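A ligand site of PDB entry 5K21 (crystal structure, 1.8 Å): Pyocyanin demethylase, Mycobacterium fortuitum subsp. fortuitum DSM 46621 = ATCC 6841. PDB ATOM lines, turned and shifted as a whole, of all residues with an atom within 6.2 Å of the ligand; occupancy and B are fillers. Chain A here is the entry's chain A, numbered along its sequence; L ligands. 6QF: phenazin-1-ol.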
ATOM      1  N   VAL A  19      35.745 -14.475   2.274  1.00  0.00           N
ATOM      2  CA  VAL A  19      34.872 -14.142   3.392  1.00  0.00           C
ATOM      3  C   VAL A  19      35.733 -13.715   4.567  1.00  0.00           C
ATOM      4  O   VAL A  19      36.614 -14.462   5.008  1.00  0.00           O
ATOM      5  CB  VAL A  19      33.988 -15.347   3.762  1.00  0.00           C
ATOM      6  CG1 VAL A  19      32.988 -14.986   4.860  1.00  0.00           C
ATOM      7  CG2 VAL A  19      33.273 -15.851   2.509  1.00  0.00           C
ATOM      8  N   ASN A  21      35.273 -12.473   8.445  1.00  0.00           N
ATOM      9  CA  ASN A  21      34.361 -12.281   9.559  1.00  0.00           C
ATOM     10  C   ASN A  21      34.379 -10.810   9.972  1.00  0.00           C
ATOM     11  O   ASN A  21      35.447 -10.198  10.084  1.00  0.00           O
ATOM     12  CB  ASN A  21      34.751 -13.150  10.759  1.00  0.00           C
ATOM     13  CG  ASN A  21      34.769 -14.630  10.433  1.00  0.00           C
ATOM     14  OD1 ASN A  21      35.579 -15.369  10.998  1.00  0.00           O
ATOM     15  ND2 ASN A  21      33.899 -15.078   9.540  1.00  0.00           N
ATOM     16  N   VAL A  24      30.885 -11.050  15.191  1.00  0.00           N
ATOM     17  CA  VAL A  24      30.413 -12.388  15.517  1.00  0.00           C
ATOM     18  C   VAL A  24      30.035 -12.420  16.985  1.00  0.00           C
ATOM     19  O   VAL A  24      30.772 -11.906  17.841  1.00  0.00           O
ATOM     20  CB  VAL A  24      31.474 -13.466  15.214  1.00  0.00           C
ATOM     21  CG1 VAL A  24      30.969 -14.826  15.621  1.00  0.00           C
ATOM     22  CG2 VAL A  24      31.832 -13.454  13.742  1.00  0.00           C
ATOM     23  N   LYS A  26      29.028 -15.486  19.680  1.00  0.00           N
ATOM     24  CA  LYS A  26      28.861 -16.908  19.932  1.00  0.00           C
ATOM     25  C   LYS A  26      28.162 -17.052  21.273  1.00  0.00           C
ATOM     26  O   LYS A  26      28.783 -16.868  22.320  1.00  0.00           O
ATOM     27  CB  LYS A  26      30.214 -17.622  19.902  1.00  0.00           C
ATOM     28  CG  LYS A  26      30.927 -17.466  18.585  1.00  0.00           C
ATOM     29  CD  LYS A  26      32.341 -17.992  18.673  1.00  0.00           C
ATOM     30  CE  LYS A  26      33.067 -17.864  17.339  1.00  0.00           C
ATOM     31  NZ  LYS A  26      34.525 -18.047  17.547  1.00  0.00           N
ATOM     32  N   ASP A  40      25.111 -18.967  17.110  1.00  0.00           N
ATOM     33  CA  ASP A  40      26.085 -18.011  16.633  1.00  0.00           C
ATOM     34  C   ASP A  40      25.391 -17.091  15.639  1.00  0.00           C
ATOM     35  O   ASP A  40      24.658 -17.542  14.748  1.00  0.00           O
ATOM     36  CB  ASP A  40      27.266 -18.691  15.961  1.00  0.00           C
ATOM     37  CG  ASP A  40      28.054 -19.570  16.930  1.00  0.00           C
ATOM     38  OD1 ASP A  40      27.785 -19.522  18.144  1.00  0.00           O
ATOM     39  OD2 ASP A  40      28.952 -20.321  16.467  1.00  0.00           O
ATOM     40  N   ILE A  41      25.659 -15.798  15.793  1.00  0.00           N
ATOM     41  CA  ILE A  41      25.114 -14.758  14.930  1.00  0.00           C
ATOM     42  C   ILE A  41      26.297 -13.971  14.377  1.00  0.00           C
ATOM     43  O   ILE A  41      27.194 -13.605  15.135  1.00  0.00           O
ATOM     44  CB  ILE A  41      24.139 -13.868  15.703  1.00  0.00           C
ATOM     45  CG1 ILE A  41      22.930 -14.705  16.120  1.00  0.00           C
ATOM     46  CG2 ILE A  41      23.709 -12.680  14.835  1.00  0.00           C
ATOM     47  CD1 ILE A  41      22.094 -14.086  17.165  1.00  0.00           C
ATOM     48  N   PHE A  42      26.293 -13.735  13.062  1.00  0.00           N
ATOM     49  CA  PHE A  42      27.507 -13.216  12.447  1.00  0.00           C
ATOM     50  C   PHE A  42      27.197 -12.380  11.220  1.00  0.00           C
ATOM     51  O   PHE A  42      26.133 -12.478  10.602  1.00  0.00           O
ATOM     52  CB  PHE A  42      28.453 -14.367  12.070  1.00  0.00           C
ATOM     53  CG  PHE A  42      27.780 -15.406  11.246  1.00  0.00           C
ATOM     54  CD1 PHE A  42      27.773 -15.302   9.853  1.00  0.00           C
ATOM     55  CD2 PHE A  42      27.106 -16.446  11.841  1.00  0.00           C
ATOM     56  CE1 PHE A  42      27.124 -16.246   9.091  1.00  0.00           C
ATOM     57  CE2 PHE A  42      26.426 -17.378  11.065  1.00  0.00           C
ATOM     58  CZ  PHE A  42      26.445 -17.276   9.708  1.00  0.00           C
ATOM     59  N   ASP A  44      29.701 -10.842   7.703  1.00  0.00           N
ATOM     60  CA  ASP A  44      30.963 -10.960   6.999  1.00  0.00           C
ATOM     61  C   ASP A  44      31.031  -9.911   5.915  1.00  0.00           C
ATOM     62  O   ASP A  44      30.024  -9.394   5.439  1.00  0.00           O
ATOM     63  CB  ASP A  44      31.150 -12.341   6.360  1.00  0.00           C
ATOM     64  CG  ASP A  44      31.008 -13.464   7.360  1.00  0.00           C
ATOM     65  OD1 ASP A  44      32.009 -13.750   8.031  1.00  0.00           O
ATOM     66  OD2 ASP A  44      29.895 -14.018   7.508  1.00  0.00           O
ATOM     67  N   ASP A  56      27.345 -10.177   4.243  1.00  0.00           N
ATOM     68  CA  ASP A  56      26.341 -11.172   4.543  1.00  0.00           C
ATOM     69  C   ASP A  56      26.028 -11.108   6.011  1.00  0.00           C
ATOM     70  O   ASP A  56      26.698 -10.417   6.797  1.00  0.00           O
ATOM     71  CB  ASP A  56      26.798 -12.582   4.097  1.00  0.00           C
ATOM     72  CG  ASP A  56      27.924 -13.149   4.938  1.00  0.00           C
ATOM     73  OD1 ASP A  56      28.007 -12.838   6.155  1.00  0.00           O
ATOM     74  OD2 ASP A  56      28.737 -13.942   4.393  1.00  0.00           O
ATOM     75  N   CYS A  60      23.249 -19.342  13.162  1.00  0.00           N
ATOM     76  CA  CYS A  60      23.316 -20.790  13.285  1.00  0.00           C
ATOM     77  C   CYS A  60      22.776 -21.202  14.643  1.00  0.00           C
ATOM     78  O   CYS A  60      23.110 -20.593  15.660  1.00  0.00           O
ATOM     79  CB  CYS A  60      24.756 -21.294  13.107  1.00  0.00           C
ATOM     80  SG  CYS A  60      25.403 -21.134  11.457  1.00  0.00           S
ATOM     81  N   PHE A  62      22.477 -24.535  17.149  1.00  0.00           N
ATOM     82  CA  PHE A  62      22.953 -25.895  17.388  1.00  0.00           C
ATOM     83  C   PHE A  62      21.766 -26.779  17.730  1.00  0.00           C
ATOM     84  O   PHE A  62      21.131 -26.614  18.768  1.00  0.00           O
ATOM     85  CB  PHE A  62      23.999 -25.937  18.510  1.00  0.00           C
ATOM     86  CG  PHE A  62      25.287 -25.322  18.131  1.00  0.00           C
ATOM     87  CD1 PHE A  62      25.447 -23.962  18.157  1.00  0.00           C
ATOM     88  CD2 PHE A  62      26.331 -26.109  17.681  1.00  0.00           C
ATOM     89  CE1 PHE A  62      26.613 -23.386  17.765  1.00  0.00           C
ATOM     90  CE2 PHE A  62      27.526 -25.533  17.298  1.00  0.00           C
ATOM     91  CZ  PHE A  62      27.673 -24.173  17.344  1.00  0.00           C
ATOM     92  N   THR A  72      24.282 -27.940  13.217  1.00  0.00           N
ATOM     93  CA  THR A  72      23.675 -26.611  13.258  1.00  0.00           C
ATOM     94  C   THR A  72      22.680 -26.458  12.124  1.00  0.00           C
ATOM     95  O   THR A  72      22.914 -26.936  11.010  1.00  0.00           O
ATOM     96  CB  THR A  72      24.708 -25.479  13.147  1.00  0.00           C
ATOM     97  OG1 THR A  72      25.548 -25.686  12.005  1.00  0.00           O
ATOM     98  CG2 THR A  72      25.562 -25.378  14.400  1.00  0.00           C
ATOM     99  N   CYS A  74      21.664 -23.522   9.983  1.00  0.00           N
ATOM    100  CA  CYS A  74      22.184 -22.207   9.643  1.00  0.00           C
ATOM    101  C   CYS A  74      21.359 -21.578   8.537  1.00  0.00           C
ATOM    102  O   CYS A  74      20.897 -22.278   7.615  1.00  0.00           O
ATOM    103  CB  CYS A  74      23.634 -22.285   9.191  1.00  0.00           C
ATOM    104  SG  CYS A  74      24.748 -22.839  10.475  1.00  0.00           S
ATOM    105  N   GLU A  75      21.179 -20.270   8.655  1.00  0.00           N
ATOM    106  CA  GLU A  75      20.551 -19.426   7.664  1.00  0.00           C
ATOM    107  C   GLU A  75      21.530 -18.326   7.310  1.00  0.00           C
ATOM    108  O   GLU A  75      22.160 -17.723   8.190  1.00  0.00           O
ATOM    109  CB  GLU A  75      19.244 -18.785   8.188  1.00  0.00           C
ATOM    110  CG  GLU A  75      18.044 -19.697   8.197  1.00  0.00           C
ATOM    111  CD  GLU A  75      17.378 -19.828   6.804  1.00  0.00           C
ATOM    112  OE1 GLU A  75      17.893 -19.240   5.820  1.00  0.00           O
ATOM    113  OE2 GLU A  75      16.366 -20.555   6.698  1.00  0.00           O
ATOM    114  N   LEU A  76      21.642 -18.058   6.014  1.00  0.00           N
ATOM    115  CA  LEU A  76      22.596 -17.079   5.524  1.00  0.00           C
ATOM    116  C   LEU A  76      21.931 -16.242   4.445  1.00  0.00           C
ATOM    117  O   LEU A  76      21.212 -16.765   3.596  1.00  0.00           O
ATOM    118  CB  LEU A  76      23.852 -17.772   4.956  1.00  0.00           C
ATOM    119  CG  LEU A  76      24.944 -16.850   4.419  1.00  0.00           C
ATOM    120  CD1 LEU A  76      25.615 -16.113   5.559  1.00  0.00           C
ATOM    121  CD2 LEU A  76      25.965 -17.692   3.683  1.00  0.00           C
ATOM    122  N   SER A  89      21.384 -24.512   5.826  1.00  0.00           N
ATOM    123  CA  SER A  89      22.073 -25.777   5.983  1.00  0.00           C
ATOM    124  C   SER A  89      21.615 -26.432   7.262  1.00  0.00           C
ATOM    125  O   SER A  89      21.175 -25.773   8.203  1.00  0.00           O
ATOM    126  CB  SER A  89      23.591 -25.573   5.987  1.00  0.00           C
ATOM    127  OG  SER A  89      23.973 -24.641   6.993  1.00  0.00           O
ATOM    128  N   HIS A  93      29.019 -28.405  12.127  1.00  0.00           N
ATOM    129  CA  HIS A  93      29.550 -27.051  12.227  1.00  0.00           C
ATOM    130  C   HIS A  93      30.974 -27.111  12.781  1.00  0.00           C
ATOM    131  O   HIS A  93      31.213 -26.794  13.945  1.00  0.00           O
ATOM    132  CB  HIS A  93      28.604 -26.222  13.081  1.00  0.00           C
ATOM    133  CG  HIS A  93      28.896 -24.767  13.084  1.00  0.00           C
ATOM    134  ND1 HIS A  93      29.588 -24.148  14.098  1.00  0.00           N
ATOM    135  CD2 HIS A  93      28.590 -23.795  12.186  1.00  0.00           C
ATOM    136  CE1 HIS A  93      29.691 -22.850  13.835  1.00  0.00           C
ATOM    137  NE2 HIS A  93      29.095 -22.615  12.686  1.00  0.00           N
ATOM    138  N   PHE A  98      31.602 -27.502   4.567  1.00  0.00           N
ATOM    139  CA  PHE A  98      30.211 -27.950   4.572  1.00  0.00           C
ATOM    140  C   PHE A  98      29.437 -27.225   3.487  1.00  0.00           C
ATOM    141  O   PHE A  98      29.825 -26.142   3.041  1.00  0.00           O
ATOM    142  CB  PHE A  98      29.542 -27.732   5.941  1.00  0.00           C
ATOM    143  CG  PHE A  98      29.499 -26.296   6.382  1.00  0.00           C
ATOM    144  CD1 PHE A  98      30.573 -25.744   7.079  1.00  0.00           C
ATOM    145  CD2 PHE A  98      28.394 -25.514   6.122  1.00  0.00           C
ATOM    146  CE1 PHE A  98      30.525 -24.427   7.485  1.00  0.00           C
ATOM    147  CE2 PHE A  98      28.345 -24.199   6.542  1.00  0.00           C
ATOM    148  CZ  PHE A  98      29.406 -23.660   7.216  1.00  0.00           C
ATOM    149  N   MET A 100      25.810 -25.705   1.896  1.00  0.00           N
ATOM    150  CA  MET A 100      24.486 -25.156   2.137  1.00  0.00           C
ATOM    151  C   MET A 100      23.650 -25.222   0.868  1.00  0.00           C
ATOM    152  O   MET A 100      24.170 -25.201  -0.257  1.00  0.00           O
ATOM    153  CB  MET A 100      24.578 -23.711   2.624  1.00  0.00           C
ATOM    154  CG  MET A 100      25.582 -23.493   3.743  1.00  0.00           C
ATOM    155  SD  MET A 100      25.544 -21.783   4.286  1.00  0.00           S
ATOM    156  CE  MET A 100      23.969 -21.733   5.125  1.00  0.00           C
ATOM    157  N   LEU A 116      26.071 -23.988  -1.883  1.00  0.00           N
ATOM    158  CA  LEU A 116      27.104 -23.065  -1.425  1.00  0.00           C
ATOM    159  C   LEU A 116      27.978 -23.812  -0.435  1.00  0.00           C
ATOM    160  O   LEU A 116      27.498 -24.237   0.619  1.00  0.00           O
ATOM    161  CB  LEU A 116      26.472 -21.830  -0.776  1.00  0.00           C
ATOM    162  CG  LEU A 116      27.370 -20.672  -0.344  1.00  0.00           C
ATOM    163  CD1 LEU A 116      26.524 -19.470  -0.076  1.00  0.00           C
ATOM    164  CD2 LEU A 116      28.181 -21.005   0.901  1.00  0.00           C
ATOM    165  N   VAL A 118      31.012 -23.841   2.164  1.00  0.00           N
ATOM    166  CA  VAL A 118      31.788 -22.986   3.068  1.00  0.00           C
ATOM    167  C   VAL A 118      33.018 -23.773   3.464  1.00  0.00           C
ATOM    168  O   VAL A 118      32.894 -24.873   4.011  1.00  0.00           O
ATOM    169  CB  VAL A 118      30.993 -22.591   4.312  1.00  0.00           C
ATOM    170  CG1 VAL A 118      31.823 -21.666   5.198  1.00  0.00           C
ATOM    171  CG2 VAL A 118      29.651 -21.952   3.970  1.00  0.00           C
ATOM    172  N   VAL A 121      35.754 -22.037   7.557  1.00  0.00           N
ATOM    173  CA  VAL A 121      34.809 -21.188   8.285  1.00  0.00           C
ATOM    174  C   VAL A 121      35.463 -20.602   9.528  1.00  0.00           C
ATOM    175  O   VAL A 121      36.151 -21.288  10.298  1.00  0.00           O
ATOM    176  CB  VAL A 121      33.546 -21.991   8.638  1.00  0.00           C
ATOM    177  CG1 VAL A 121      33.832 -23.103   9.647  1.00  0.00           C
ATOM    178  CG2 VAL A 121      32.444 -21.078   9.141  1.00  0.00           C
ATOM    179  N   ALA A 122      35.242 -19.298   9.721  1.00  0.00           N
ATOM    180  CA  ALA A 122      35.755 -18.537  10.860  1.00  0.00           C
ATOM    181  C   ALA A 122      37.281 -18.529  10.915  1.00  0.00           C
ATOM    182  O   ALA A 122      37.864 -18.342  11.995  1.00  0.00           O
ATOM    183  CB  ALA A 122      35.197 -19.053  12.184  1.00  0.00           C
ATOM    184  N   GLU A 126      38.563 -18.113   4.888  1.00  0.00           N
ATOM    185  CA  GLU A 126      37.211 -18.582   4.630  1.00  0.00           C
ATOM    186  C   GLU A 126      36.804 -18.213   3.202  1.00  0.00           C
ATOM    187  O   GLU A 126      37.107 -17.130   2.715  1.00  0.00           O
ATOM    188  CB  GLU A 126      36.237 -17.974   5.643  1.00  0.00           C
ATOM    189  CG  GLU A 126      34.808 -18.515   5.543  1.00  0.00           C
ATOM    190  CD  GLU A 126      33.891 -17.996   6.636  1.00  0.00           C
ATOM    191  OE1 GLU A 126      34.392 -17.504   7.673  1.00  0.00           O
ATOM    192  OE2 GLU A 126      32.661 -18.111   6.460  1.00  0.00           O
ATOM    193  N   TYR A 128      33.439 -18.943   0.197  1.00  0.00           N
ATOM    194  CA  TYR A 128      32.192 -19.540  -0.254  1.00  0.00           C
ATOM    195  C   TYR A 128      32.373 -19.914  -1.723  1.00  0.00           C
ATOM    196  O   TYR A 128      32.812 -19.096  -2.522  1.00  0.00           O
ATOM    197  CB  TYR A 128      30.995 -18.595  -0.145  1.00  0.00           C
ATOM    198  CG  TYR A 128      30.653 -18.038   1.226  1.00  0.00           C
ATOM    199  CD1 TYR A 128      30.985 -18.707   2.401  1.00  0.00           C
ATOM    200  CD2 TYR A 128      29.965 -16.839   1.319  1.00  0.00           C
ATOM    201  CE1 TYR A 128      30.652 -18.165   3.637  1.00  0.00           C
ATOM    202  CE2 TYR A 128      29.634 -16.295   2.540  1.00  0.00           C
ATOM    203  CZ  TYR A 128      29.978 -16.963   3.695  1.00  0.00           C
ATOM    204  OH  TYR A 128      29.640 -16.411   4.902  1.00  0.00           O
HETATM  205  C4  6QF L   1      29.706 -19.092  11.384  1.00  0.00           C
HETATM  206  C5  6QF L   1      30.050 -19.053  12.817  1.00  0.00           C
HETATM  207  C6  6QF L   1      30.931 -18.160  13.325  1.00  0.00           C
HETATM  208  C10 6QF L   1      29.174 -19.004   8.698  1.00  0.00           C
HETATM  209  C13 6QF L   1      27.917 -19.943   6.805  1.00  0.00           C
HETATM  210  C15 6QF L   1      27.614 -20.904   8.959  1.00  0.00           C
HETATM  211  C1  6QF L   1      31.552 -17.208  12.453  1.00  0.00           C
HETATM  212  C2  6QF L   1      31.264 -17.195  11.151  1.00  0.00           C
HETATM  213  C3  6QF L   1      30.327 -18.112  10.522  1.00  0.00           C
HETATM  214  N7  6QF L   1      30.058 -18.093   9.194  1.00  0.00           N
HETATM  215  N8  6QF L   1      28.832 -19.992  10.876  1.00  0.00           N
HETATM  216  C9  6QF L   1      28.563 -19.974   9.562  1.00  0.00           C
HETATM  217  C11 6QF L   1      28.789 -19.059   7.297  1.00  0.00           C
HETATM  218  C14 6QF L   1      27.291 -20.899   7.669  1.00  0.00           C
HETATM  219  O19 6QF L   1      29.451 -19.964  13.617  1.00  0.00           O
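An oxygen (O19) of the ligand lies within hydrogen-bond range of a ring nitrogen (NE2) of His 93 (2.8 Å).
The side-chain carboxylate (OD2) of Asp 40 lies within hydrogen-bond range of an oxygen (O19) of the ligand, at 2.9 Å.
O of Asp 40 is in hydrogen-bond range of N of Cys 60, 2.8 Å away.
SG of Cys 60 is disulfide-bonded to SG of Cys 74 (2.1 Å).
ND2 of Asn 21 lies within hydrogen-bond range of OD1 of Asp 44, at 2.8 Å.
OE1 of Glu 126 lies within hydrogen-bond range of N of Ala 122 (2.9 Å).
The backbone carbonyl oxygen (O) of Glu 126 lies within hydrogen-bond range of the backbone NH (N) of Val 19, 3.0 Å away.
The backbone carbonyl oxygen of Cys 74 is in hydrogen-bond range of the backbone NH of Ser 89, 2.9 Å away.
The side-chain hydroxyl (OG1) of Thr 72 is in hydrogen-bond range of the side-chain sulfur (SG) of Cys 74 (3.3 Å).
N of Met 100 sits at hydrogen-bond distance from O of Leu 116.
The side-chain sulfur (SG) of Cys 60 sits close to a nitrogen (N8) of the ligand, at 3.7 Å.
ND2 of Asn 21 touches C2 of the ligand (3.7 Å).
Val 24 touches the ligand (CG2 to C1, 3.98 Å).
Phe 42 touches the ligand.
Cys 74 touches the ligand.
Phe 98 touches the ligand (CZ to C14, 3.5 Å).
SD of Met 100 touches C14 of the ligand, at 3.9 Å.
Val 118 touches the ligand (CG2 to C13, 3.9 Å).
Val 121 touches the ligand (CG2 to N7, 3.8 Å).
OE2 of Glu 126 touches N7 of the ligand, 3.8 Å away.
OH of Tyr 128 touches C11 of the ligand, 3.7 Å away.
Hydrophobic or aromatic side chains within 4 Å of the ligand: Val 24, Phe 42, His 93, Phe 98, Met 100, Val 118 and Val 121.
13 residues have an atom within 4 Å of the ligand: Asn 21, Val 24, Asp 40, Phe 42, Cys 60, Cys 74, His 93, Phe 98, Met 100, Val 118, Val 121, Glu 126 and Tyr 128.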
